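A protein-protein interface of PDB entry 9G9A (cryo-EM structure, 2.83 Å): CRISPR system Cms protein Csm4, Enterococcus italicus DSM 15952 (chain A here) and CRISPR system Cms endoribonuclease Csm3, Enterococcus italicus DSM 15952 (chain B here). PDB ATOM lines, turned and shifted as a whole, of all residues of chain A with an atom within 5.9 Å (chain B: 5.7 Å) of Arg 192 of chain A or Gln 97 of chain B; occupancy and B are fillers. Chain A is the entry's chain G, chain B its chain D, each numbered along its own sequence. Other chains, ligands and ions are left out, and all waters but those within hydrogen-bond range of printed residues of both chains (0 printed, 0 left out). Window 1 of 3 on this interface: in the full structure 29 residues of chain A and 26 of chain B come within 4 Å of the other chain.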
ATOM      1  N   TYR A 185       3.179  -6.755   9.323  1.00  0.00           N
ATOM      2  CA  TYR A 185       2.950  -7.599  10.483  1.00  0.00           C
ATOM      3  C   TYR A 185       1.704  -7.214  11.264  1.00  0.00           C
ATOM      4  O   TYR A 185       1.186  -8.045  12.018  1.00  0.00           O
ATOM      5  CB  TYR A 185       4.170  -7.553  11.406  1.00  0.00           C
ATOM      6  CG  TYR A 185       5.470  -7.694  10.652  1.00  0.00           C
ATOM      7  CD1 TYR A 185       5.930  -8.939  10.250  1.00  0.00           C
ATOM      8  CD2 TYR A 185       6.228  -6.581  10.327  1.00  0.00           C
ATOM      9  CE1 TYR A 185       7.113  -9.071   9.554  1.00  0.00           C
ATOM     10  CE2 TYR A 185       7.413  -6.703   9.630  1.00  0.00           C
ATOM     11  CZ  TYR A 185       7.851  -7.950   9.247  1.00  0.00           C
ATOM     12  OH  TYR A 185       9.032  -8.077   8.553  1.00  0.00           O
ATOM     13  N   SER A 186       1.210  -5.983  11.106  1.00  0.00           N
ATOM     14  CA  SER A 186      -0.079  -5.629  11.693  1.00  0.00           C
ATOM     15  C   SER A 186      -1.223  -6.322  10.960  1.00  0.00           C
ATOM     16  O   SER A 186      -2.149  -6.842  11.589  1.00  0.00           O
ATOM     17  CB  SER A 186      -0.269  -4.113  11.677  1.00  0.00           C
ATOM     18  OG  SER A 186      -1.520  -3.747  12.230  1.00  0.00           O
ATOM     19  N   GLY A 187      -1.170  -6.340   9.634  1.00  0.00           N
ATOM     20  CA  GLY A 187      -2.157  -7.023   8.829  1.00  0.00           C
ATOM     21  C   GLY A 187      -3.309  -6.120   8.421  1.00  0.00           C
ATOM     22  O   GLY A 187      -3.564  -5.071   9.011  1.00  0.00           O
ATOM     23  N   ILE A 188      -4.018  -6.551   7.381  1.00  0.00           N
ATOM     24  CA  ILE A 188      -5.223  -5.882   6.908  1.00  0.00           C
ATOM     25  C   ILE A 188      -6.340  -6.911   6.848  1.00  0.00           C
ATOM     26  O   ILE A 188      -6.104  -8.074   6.502  1.00  0.00           O
ATOM     27  CB  ILE A 188      -5.022  -5.216   5.533  1.00  0.00           C
ATOM     28  CG1 ILE A 188      -4.586  -6.241   4.485  1.00  0.00           C
ATOM     29  CG2 ILE A 188      -4.022  -4.078   5.630  1.00  0.00           C
ATOM     30  CD1 ILE A 188      -4.509  -5.679   3.085  1.00  0.00           C
ATOM     31  N   GLY A 189      -7.541  -6.491   7.194  1.00  0.00           N
ATOM     32  CA  GLY A 189      -8.695  -7.357   7.068  1.00  0.00           C
ATOM     33  C   GLY A 189      -9.494  -7.375   8.353  1.00  0.00           C
ATOM     34  O   GLY A 189      -9.270  -6.593   9.270  1.00  0.00           O
ATOM     35  N   GLY A 190     -10.439  -8.306   8.398  1.00  0.00           N
ATOM     36  CA  GLY A 190     -11.356  -8.380   9.514  1.00  0.00           C
ATOM     37  C   GLY A 190     -11.089  -9.459  10.527  1.00  0.00           C
ATOM     38  O   GLY A 190     -11.906  -9.655  11.429  1.00  0.00           O
ATOM     39  N   LYS A 191      -9.991 -10.199  10.388  1.00  0.00           N
ATOM     40  CA  LYS A 191      -9.597 -11.205  11.369  1.00  0.00           C
ATOM     41  C   LYS A 191      -8.096 -11.183  11.630  1.00  0.00           C
ATOM     42  O   LYS A 191      -7.466 -12.241  11.694  1.00  0.00           O
ATOM     43  CB  LYS A 191     -10.047 -12.591  10.914  1.00  0.00           C
ATOM     44  CG  LYS A 191     -10.789 -13.387  11.973  1.00  0.00           C
ATOM     45  CD  LYS A 191     -12.040 -12.673  12.448  1.00  0.00           C
ATOM     46  CE  LYS A 191     -12.687 -13.418  13.607  1.00  0.00           C
ATOM     47  NZ  LYS A 191     -13.812 -12.655  14.209  1.00  0.00           N
ATOM     48  N   ARG A 192      -7.512  -9.992  11.771  1.00  0.00           N
ATOM     49  CA  ARG A 192      -6.061  -9.864  11.842  1.00  0.00           C
ATOM     50  C   ARG A 192      -5.490 -10.561  13.069  1.00  0.00           C
ATOM     51  O   ARG A 192      -4.438 -11.206  13.001  1.00  0.00           O
ATOM     52  CB  ARG A 192      -5.677  -8.385  11.843  1.00  0.00           C
ATOM     53  CG  ARG A 192      -6.321  -7.595  10.728  1.00  0.00           C
ATOM     54  CD  ARG A 192      -6.000  -6.119  10.829  1.00  0.00           C
ATOM     55  NE  ARG A 192      -6.455  -5.534  12.082  1.00  0.00           N
ATOM     56  CZ  ARG A 192      -5.656  -5.218  13.092  1.00  0.00           C
ATOM     57  NH1 ARG A 192      -4.349  -5.407  13.023  1.00  0.00           N
ATOM     58  NH2 ARG A 192      -6.180  -4.700  14.197  1.00  0.00           N
ATOM     59  N   SER A 193      -6.169 -10.427  14.209  1.00  0.00           N
ATOM     60  CA  SER A 193      -5.655 -11.012  15.441  1.00  0.00           C
ATOM     61  C   SER A 193      -5.986 -12.495  15.532  1.00  0.00           C
ATOM     62  O   SER A 193      -5.469 -13.201  16.407  1.00  0.00           O
ATOM     63  CB  SER A 193      -6.219 -10.261  16.646  1.00  0.00           C
ATOM     64  OG  SER A 193      -5.849  -8.894  16.610  1.00  0.00           O
ATOM     65  N   ALA A 194      -6.844 -12.989  14.644  1.00  0.00           N
ATOM     66  CA  ALA A 194      -7.260 -14.382  14.671  1.00  0.00           C
ATOM     67  C   ALA A 194      -6.713 -15.197  13.503  1.00  0.00           C
ATOM     68  O   ALA A 194      -7.228 -16.286  13.235  1.00  0.00           O
ATOM     69  CB  ALA A 194      -8.785 -14.476  14.701  1.00  0.00           C
ATOM     70  N   GLY A 195      -5.694 -14.706  12.805  1.00  0.00           N
ATOM     71  CA  GLY A 195      -4.975 -15.515  11.844  1.00  0.00           C
ATOM     72  C   GLY A 195      -5.153 -15.177  10.381  1.00  0.00           C
ATOM     73  O   GLY A 195      -4.644 -15.917   9.533  1.00  0.00           O
ATOM     74  N   TYR A 196      -5.842 -14.093  10.053  1.00  0.00           N
ATOM     75  CA  TYR A 196      -6.075 -13.723   8.666  1.00  0.00           C
ATOM     76  C   TYR A 196      -5.460 -12.361   8.371  1.00  0.00           C
ATOM     77  O   TYR A 196      -5.434 -11.480   9.234  1.00  0.00           O
ATOM     78  CB  TYR A 196      -7.573 -13.700   8.356  1.00  0.00           C
ATOM     79  CG  TYR A 196      -8.226 -15.066   8.353  1.00  0.00           C
ATOM     80  CD1 TYR A 196      -7.554 -16.178   7.875  1.00  0.00           C
ATOM     81  CD2 TYR A 196      -9.514 -15.240   8.829  1.00  0.00           C
ATOM     82  CE1 TYR A 196      -8.150 -17.423   7.868  1.00  0.00           C
ATOM     83  CE2 TYR A 196     -10.116 -16.480   8.829  1.00  0.00           C
ATOM     84  CZ  TYR A 196      -9.430 -17.569   8.348  1.00  0.00           C
ATOM     85  OH  TYR A 196     -10.024 -18.809   8.344  1.00  0.00           O
ATOM     86  N   GLY A 197      -4.958 -12.195   7.152  1.00  0.00           N
ATOM     87  CA  GLY A 197      -4.544 -10.890   6.679  1.00  0.00           C
ATOM     88  C   GLY A 197      -3.063 -10.589   6.719  1.00  0.00           C
ATOM     89  O   GLY A 197      -2.677  -9.464   6.388  1.00  0.00           O
ATOM     90  N   GLN A 198      -2.223 -11.540   7.115  1.00  0.00           N
ATOM     91  CA  GLN A 198      -0.787 -11.307   7.086  1.00  0.00           C
ATOM     92  C   GLN A 198      -0.290 -11.229   5.646  1.00  0.00           C
ATOM     93  O   GLN A 198      -0.719 -11.988   4.774  1.00  0.00           O
ATOM     94  CB  GLN A 198      -0.048 -12.409   7.844  1.00  0.00           C
ATOM     95  CG  GLN A 198      -0.167 -12.306   9.357  1.00  0.00           C
ATOM     96  CD  GLN A 198       0.566 -11.104   9.921  1.00  0.00           C
ATOM     97  OE1 GLN A 198       1.529 -10.615   9.332  1.00  0.00           O
ATOM     98  NE2 GLN A 198       0.112 -10.620  11.070  1.00  0.00           N
ATOM     99  N   GLN A 252     -13.112   1.210  15.225  1.00  0.00           N
ATOM    100  CA  GLN A 252     -12.106   0.308  15.779  1.00  0.00           C
ATOM    101  C   GLN A 252     -11.038   1.149  16.472  1.00  0.00           C
ATOM    102  O   GLN A 252     -10.109   1.644  15.827  1.00  0.00           O
ATOM    103  CB  GLN A 252     -11.497  -0.572  14.692  1.00  0.00           C
ATOM    104  CG  GLN A 252     -10.372  -1.468  15.180  1.00  0.00           C
ATOM    105  CD  GLN A 252      -9.739  -2.271  14.063  1.00  0.00           C
ATOM    106  OE1 GLN A 252     -10.431  -2.885  13.254  1.00  0.00           O
ATOM    107  NE2 GLN A 252      -8.414  -2.265  14.009  1.00  0.00           N
ATOM    108  N   LYS B   4       7.045  -4.784  17.355  1.00  0.00           N
ATOM    109  CA  LYS B   4       6.408  -6.049  17.021  1.00  0.00           C
ATOM    110  C   LYS B   4       7.482  -7.118  16.919  1.00  0.00           C
ATOM    111  O   LYS B   4       8.507  -6.910  16.261  1.00  0.00           O
ATOM    112  CB  LYS B   4       5.610  -5.949  15.719  1.00  0.00           C
ATOM    113  CG  LYS B   4       4.123  -5.731  15.940  1.00  0.00           C
ATOM    114  CD  LYS B   4       3.411  -5.307  14.669  1.00  0.00           C
ATOM    115  CE  LYS B   4       3.735  -3.869  14.313  1.00  0.00           C
ATOM    116  NZ  LYS B   4       2.948  -3.402  13.142  1.00  0.00           N
ATOM    117  N   SER B  93      -6.611  -4.181  22.598  1.00  0.00           N
ATOM    118  CA  SER B  93      -6.156  -4.790  21.357  1.00  0.00           C
ATOM    119  C   SER B  93      -5.375  -6.065  21.649  1.00  0.00           C
ATOM    120  O   SER B  93      -4.595  -6.129  22.602  1.00  0.00           O
ATOM    121  CB  SER B  93      -5.290  -3.808  20.570  1.00  0.00           C
ATOM    122  OG  SER B  93      -4.856  -4.376  19.347  1.00  0.00           O
ATOM    123  N   SER B  94      -5.589  -7.083  20.820  1.00  0.00           N
ATOM    124  CA  SER B  94      -4.918  -8.361  21.013  1.00  0.00           C
ATOM    125  C   SER B  94      -3.433  -8.239  20.704  1.00  0.00           C
ATOM    126  O   SER B  94      -3.049  -7.839  19.601  1.00  0.00           O
ATOM    127  CB  SER B  94      -5.560  -9.425  20.127  1.00  0.00           C
ATOM    128  OG  SER B  94      -4.914 -10.674  20.285  1.00  0.00           O
ATOM    129  N   ARG B  95      -2.597  -8.583  21.686  1.00  0.00           N
ATOM    130  CA  ARG B  95      -1.153  -8.551  21.483  1.00  0.00           C
ATOM    131  C   ARG B  95      -0.673  -9.750  20.676  1.00  0.00           C
ATOM    132  O   ARG B  95       0.317  -9.651  19.944  1.00  0.00           O
ATOM    133  CB  ARG B  95      -0.431  -8.495  22.828  1.00  0.00           C
ATOM    134  CG  ARG B  95      -0.684  -7.225  23.613  1.00  0.00           C
ATOM    135  CD  ARG B  95       0.134  -7.197  24.889  1.00  0.00           C
ATOM    136  NE  ARG B  95      -0.115  -5.987  25.663  1.00  0.00           N
ATOM    137  CZ  ARG B  95       0.555  -5.644  26.752  1.00  0.00           C
ATOM    138  NH1 ARG B  95       1.535  -6.394  27.228  1.00  0.00           N
ATOM    139  NH2 ARG B  95       0.237  -4.516  27.381  1.00  0.00           N
ATOM    140  N   LEU B  96      -1.351 -10.889  20.797  1.00  0.00           N
ATOM    141  CA  LEU B  96      -0.962 -12.107  20.094  1.00  0.00           C
ATOM    142  C   LEU B  96      -1.767 -12.228  18.807  1.00  0.00           C
ATOM    143  O   LEU B  96      -2.988 -12.418  18.844  1.00  0.00           O
ATOM    144  CB  LEU B  96      -1.173 -13.334  20.975  1.00  0.00           C
ATOM    145  CG  LEU B  96      -0.061 -13.685  21.961  1.00  0.00           C
ATOM    146  CD1 LEU B  96      -0.397 -14.965  22.697  1.00  0.00           C
ATOM    147  CD2 LEU B  96       1.264 -13.813  21.233  1.00  0.00           C
ATOM    148  N   GLN B  97      -1.087 -12.122  17.671  1.00  0.00           N
ATOM    149  CA  GLN B  97      -1.666 -12.413  16.368  1.00  0.00           C
ATOM    150  C   GLN B  97      -1.069 -13.724  15.875  1.00  0.00           C
ATOM    151  O   GLN B  97       0.080 -13.754  15.424  1.00  0.00           O
ATOM    152  CB  GLN B  97      -1.389 -11.282  15.380  1.00  0.00           C
ATOM    153  CG  GLN B  97      -1.842  -9.919  15.862  1.00  0.00           C
ATOM    154  CD  GLN B  97      -1.543  -8.821  14.863  1.00  0.00           C
ATOM    155  OE1 GLN B  97      -0.516  -8.152  14.950  1.00  0.00           O
ATOM    156  NE2 GLN B  97      -2.443  -8.630  13.907  1.00  0.00           N
ATOM    157  N   ILE B  98      -1.836 -14.804  15.987  1.00  0.00           N
ATOM    158  CA  ILE B  98      -1.383 -16.140  15.619  1.00  0.00           C
ATOM    159  C   ILE B  98      -1.973 -16.472  14.258  1.00  0.00           C
ATOM    160  O   ILE B  98      -3.197 -16.577  14.115  1.00  0.00           O
ATOM    161  CB  ILE B  98      -1.792 -17.186  16.666  1.00  0.00           C
ATOM    162  CG1 ILE B  98      -1.317 -16.756  18.055  1.00  0.00           C
ATOM    163  CG2 ILE B  98      -1.233 -18.548  16.302  1.00  0.00           C
ATOM    164  CD1 ILE B  98      -1.814 -17.643  19.169  1.00  0.00           C
ATOM    165  N   SER B  99      -1.106 -16.653  13.267  1.00  0.00           N
ATOM    166  CA  SER B  99      -1.560 -16.907  11.909  1.00  0.00           C
ATOM    167  C   SER B  99      -1.864 -18.386  11.704  1.00  0.00           C
ATOM    168  O   SER B  99      -1.534 -19.235  12.539  1.00  0.00           O
ATOM    169  CB  SER B  99      -0.506 -16.451  10.903  1.00  0.00           C
ATOM    170  OG  SER B  99      -0.188 -15.083  11.093  1.00  0.00           O
ATOM    171  N   HIS B 151       3.536 -19.046  12.661  1.00  0.00           N
ATOM    172  CA  HIS B 151       4.028 -17.674  12.620  1.00  0.00           C
ATOM    173  C   HIS B 151       3.176 -16.849  13.573  1.00  0.00           C
ATOM    174  O   HIS B 151       1.956 -16.772  13.401  1.00  0.00           O
ATOM    175  CB  HIS B 151       3.951 -17.127  11.192  1.00  0.00           C
ATOM    176  CG  HIS B 151       4.266 -15.668  11.073  1.00  0.00           C
ATOM    177  ND1 HIS B 151       3.325 -14.685  11.290  1.00  0.00           N
ATOM    178  CD2 HIS B 151       5.408 -15.028  10.730  1.00  0.00           C
ATOM    179  CE1 HIS B 151       3.879 -13.501  11.102  1.00  0.00           C
ATOM    180  NE2 HIS B 151       5.142 -13.681  10.760  1.00  0.00           N
ATOM    181  N   ILE B 152       3.808 -16.249  14.577  1.00  0.00           N
ATOM    182  CA  ILE B 152       3.113 -15.499  15.615  1.00  0.00           C
ATOM    183  C   ILE B 152       3.716 -14.105  15.696  1.00  0.00           C
ATOM    184  O   ILE B 152       4.927 -13.923  15.540  1.00  0.00           O
ATOM    185  CB  ILE B 152       3.197 -16.215  16.984  1.00  0.00           C
ATOM    186  CG1 ILE B 152       2.620 -17.627  16.889  1.00  0.00           C
ATOM    187  CG2 ILE B 152       2.470 -15.425  18.060  1.00  0.00           C
ATOM    188  CD1 ILE B 152       2.622 -18.376  18.204  1.00  0.00           C
ATOM    189  N   ILE B 153       2.862 -13.112  15.929  1.00  0.00           N
ATOM    190  CA  ILE B 153       3.286 -11.732  16.121  1.00  0.00           C
ATOM    191  C   ILE B 153       2.874 -11.297  17.519  1.00  0.00           C
ATOM    192  O   ILE B 153       1.712 -11.457  17.907  1.00  0.00           O
ATOM    193  CB  ILE B 153       2.680 -10.794  15.060  1.00  0.00           C
ATOM    194  CG1 ILE B 153       3.235 -11.126  13.676  1.00  0.00           C
ATOM    195  CG2 ILE B 153       2.963  -9.342  15.405  1.00  0.00           C
ATOM    196  CD1 ILE B 153       4.687 -10.760  13.501  1.00  0.00           C
ATOM    197  N   TYR B 154       3.825 -10.760  18.274  1.00  0.00           N
ATOM    198  CA  TYR B 154       3.545 -10.154  19.567  1.00  0.00           C
ATOM    199  C   TYR B 154       3.670  -8.645  19.434  1.00  0.00           C
ATOM    200  O   TYR B 154       4.667  -8.144  18.903  1.00  0.00           O
ATOM    201  CB  TYR B 154       4.494 -10.672  20.649  1.00  0.00           C
ATOM    202  CG  TYR B 154       4.262 -10.037  22.001  1.00  0.00           C
ATOM    203  CD1 TYR B 154       3.284 -10.521  22.859  1.00  0.00           C
ATOM    204  CD2 TYR B 154       5.015  -8.948  22.418  1.00  0.00           C
ATOM    205  CE1 TYR B 154       3.067  -9.940  24.093  1.00  0.00           C
ATOM    206  CE2 TYR B 154       4.803  -8.361  23.649  1.00  0.00           C
ATOM    207  CZ  TYR B 154       3.829  -8.860  24.482  1.00  0.00           C
ATOM    208  OH  TYR B 154       3.615  -8.280  25.710  1.00  0.00           O
ATOM    209  N   ASN B 155       2.665  -7.926  19.921  1.00  0.00           N
ATOM    210  CA  ASN B 155       2.640  -6.472  19.867  1.00  0.00           C
ATOM    211  C   ASN B 155       3.081  -5.923  21.217  1.00  0.00           C
ATOM    212  O   ASN B 155       2.430  -6.179  22.235  1.00  0.00           O
ATOM    213  CB  ASN B 155       1.242  -5.969  19.509  1.00  0.00           C
ATOM    214  CG  ASN B 155       0.756  -6.490  18.170  1.00  0.00           C
ATOM    215  OD1 ASN B 155       0.147  -7.556  18.089  1.00  0.00           O
ATOM    216  ND2 ASN B 155       1.020  -5.737  17.111  1.00  0.00           N
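The backbone carbonyl oxygen (O) of Ile 98 of chain B sits close to the backbone NH (N) of Gly 195 of chain A (3.4 Å).
The side-chain amide oxygen (OE1) of Gln 97 of chain B lies close to the backbone carbonyl oxygen (O) of Tyr 185 of chain A (3.4 Å).
NE2 of Gln 97 of chain B is in hydrogen-bond range of O of Arg 192 of chain A (3.4 Å).
NE2 of Gln 97 of chain B sits at hydrogen-bond distance from O of Ser 186 of chain A (2.9 Å).
Of the 15 printed residues of chain A, 7 touch a printed residue of chain B.
Hydrophobic or aromatic side chains of chain A within 4 Å of the printed part of chain B: Tyr 185.
Printed residues of chain B that touch a printed residue of chain A: Lys 4, Ser 94, Leu 96, Gln 97, Ile 98, Ser 99 and Ile 153.
Hydrophobic or aromatic side chains of chain B within 4 Å of the printed part of chain A: Ile 153.
Among the printed residues, 13 pairs touch across the chains.
Among the printed residues, no Asp or Glu carboxylate lies within 4 Å of a Lys or Arg side-chain nitrogen of the other chain.
Arg 192 of chain A touches just one residue of chain B: Gln 97.
Of the printed residues of chain B, Ser 193 of chain A touches Ser 94 (3.6 Å), Leu 96 (3.6 Å), Gln 97 (3.9 Å) and Ile 98 (3.99 Å).
Of the printed residues of chain B, Ala 194 of chain A touches Ile 98.
Printed residues of chain A within 4 Å of Ser 94 of chain B: Ser 193 (3.6 Å).
Printed residues of chain A within 4 Å of Leu 96 of chain B: Ser 193 (3.6 Å).
Of chain A, only Tyr 185, Ser 186, Arg 192 and Ser 193 come within 4 Å of Gln 97 of chain B.
Of the printed residues of chain A, Ile 98 of chain B touches Ser 193, Ala 194 and Gly 195.
The nearest residue of chain A that does not touch Gln 97 of chain B is Gln 198 of chain A (4.3 Å).
The nearest printed residue of chain A that does not touch Ser 94 of chain B is Ala 194 of chain A (6.4 Å).
Among the printed residues, pairs that only touch across the chains: Gln 198 of chain A with Ser 99 of chain B (3.3 Å), Ser 193 of chain A with Leu 96 of chain B (3.6 Å), Ser 193 of chain A with Ser 94 of chain B (3.6 Å), Ser 186 of chain A with Lys 4 of chain B (3.6 Å), Gly 195 of chain A with Ser 99 of chain B (3.7 Å), Ala 194 of chain A with Ile 98 of chain B (3.8 Å), Tyr 185 of chain A with Ile 153 of chain B (3.9 Å), Ser 193 of chain A with Gln 97 of chain B (3.9 Å) and Ser 193 of chain A with Ile 98 of chain B (3.99 Å).
The backbone NH of Gln 97 of chain B lies within hydrogen-bond range of the backbone carbonyl oxygen of Ile 153 of chain B.
The side-chain amide oxygen of Asn 155 of chain B sits close to the side-chain amide oxygen of Gln 97 of chain B, at 3.3 Å.
OG of Ser 94 of chain B lies within hydrogen-bond range of O of Leu 96 of chain B, at 3.0 Å.
The backbone NH (N) of Ser 99 of chain B sits at hydrogen-bond distance from the backbone carbonyl oxygen (O) of His 151 of chain B (3.1 Å).
The side-chain amide nitrogen of Gln 252 of chain A lies close to the guanidinium group of Arg 192 of chain A, at 3.3 Å.
The backbone carbonyl oxygen (O) of Ser 186 of chain A sits at hydrogen-bond distance from the guanidinium group (NH1) of Arg 192 of chain A, 3.0 Å away.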
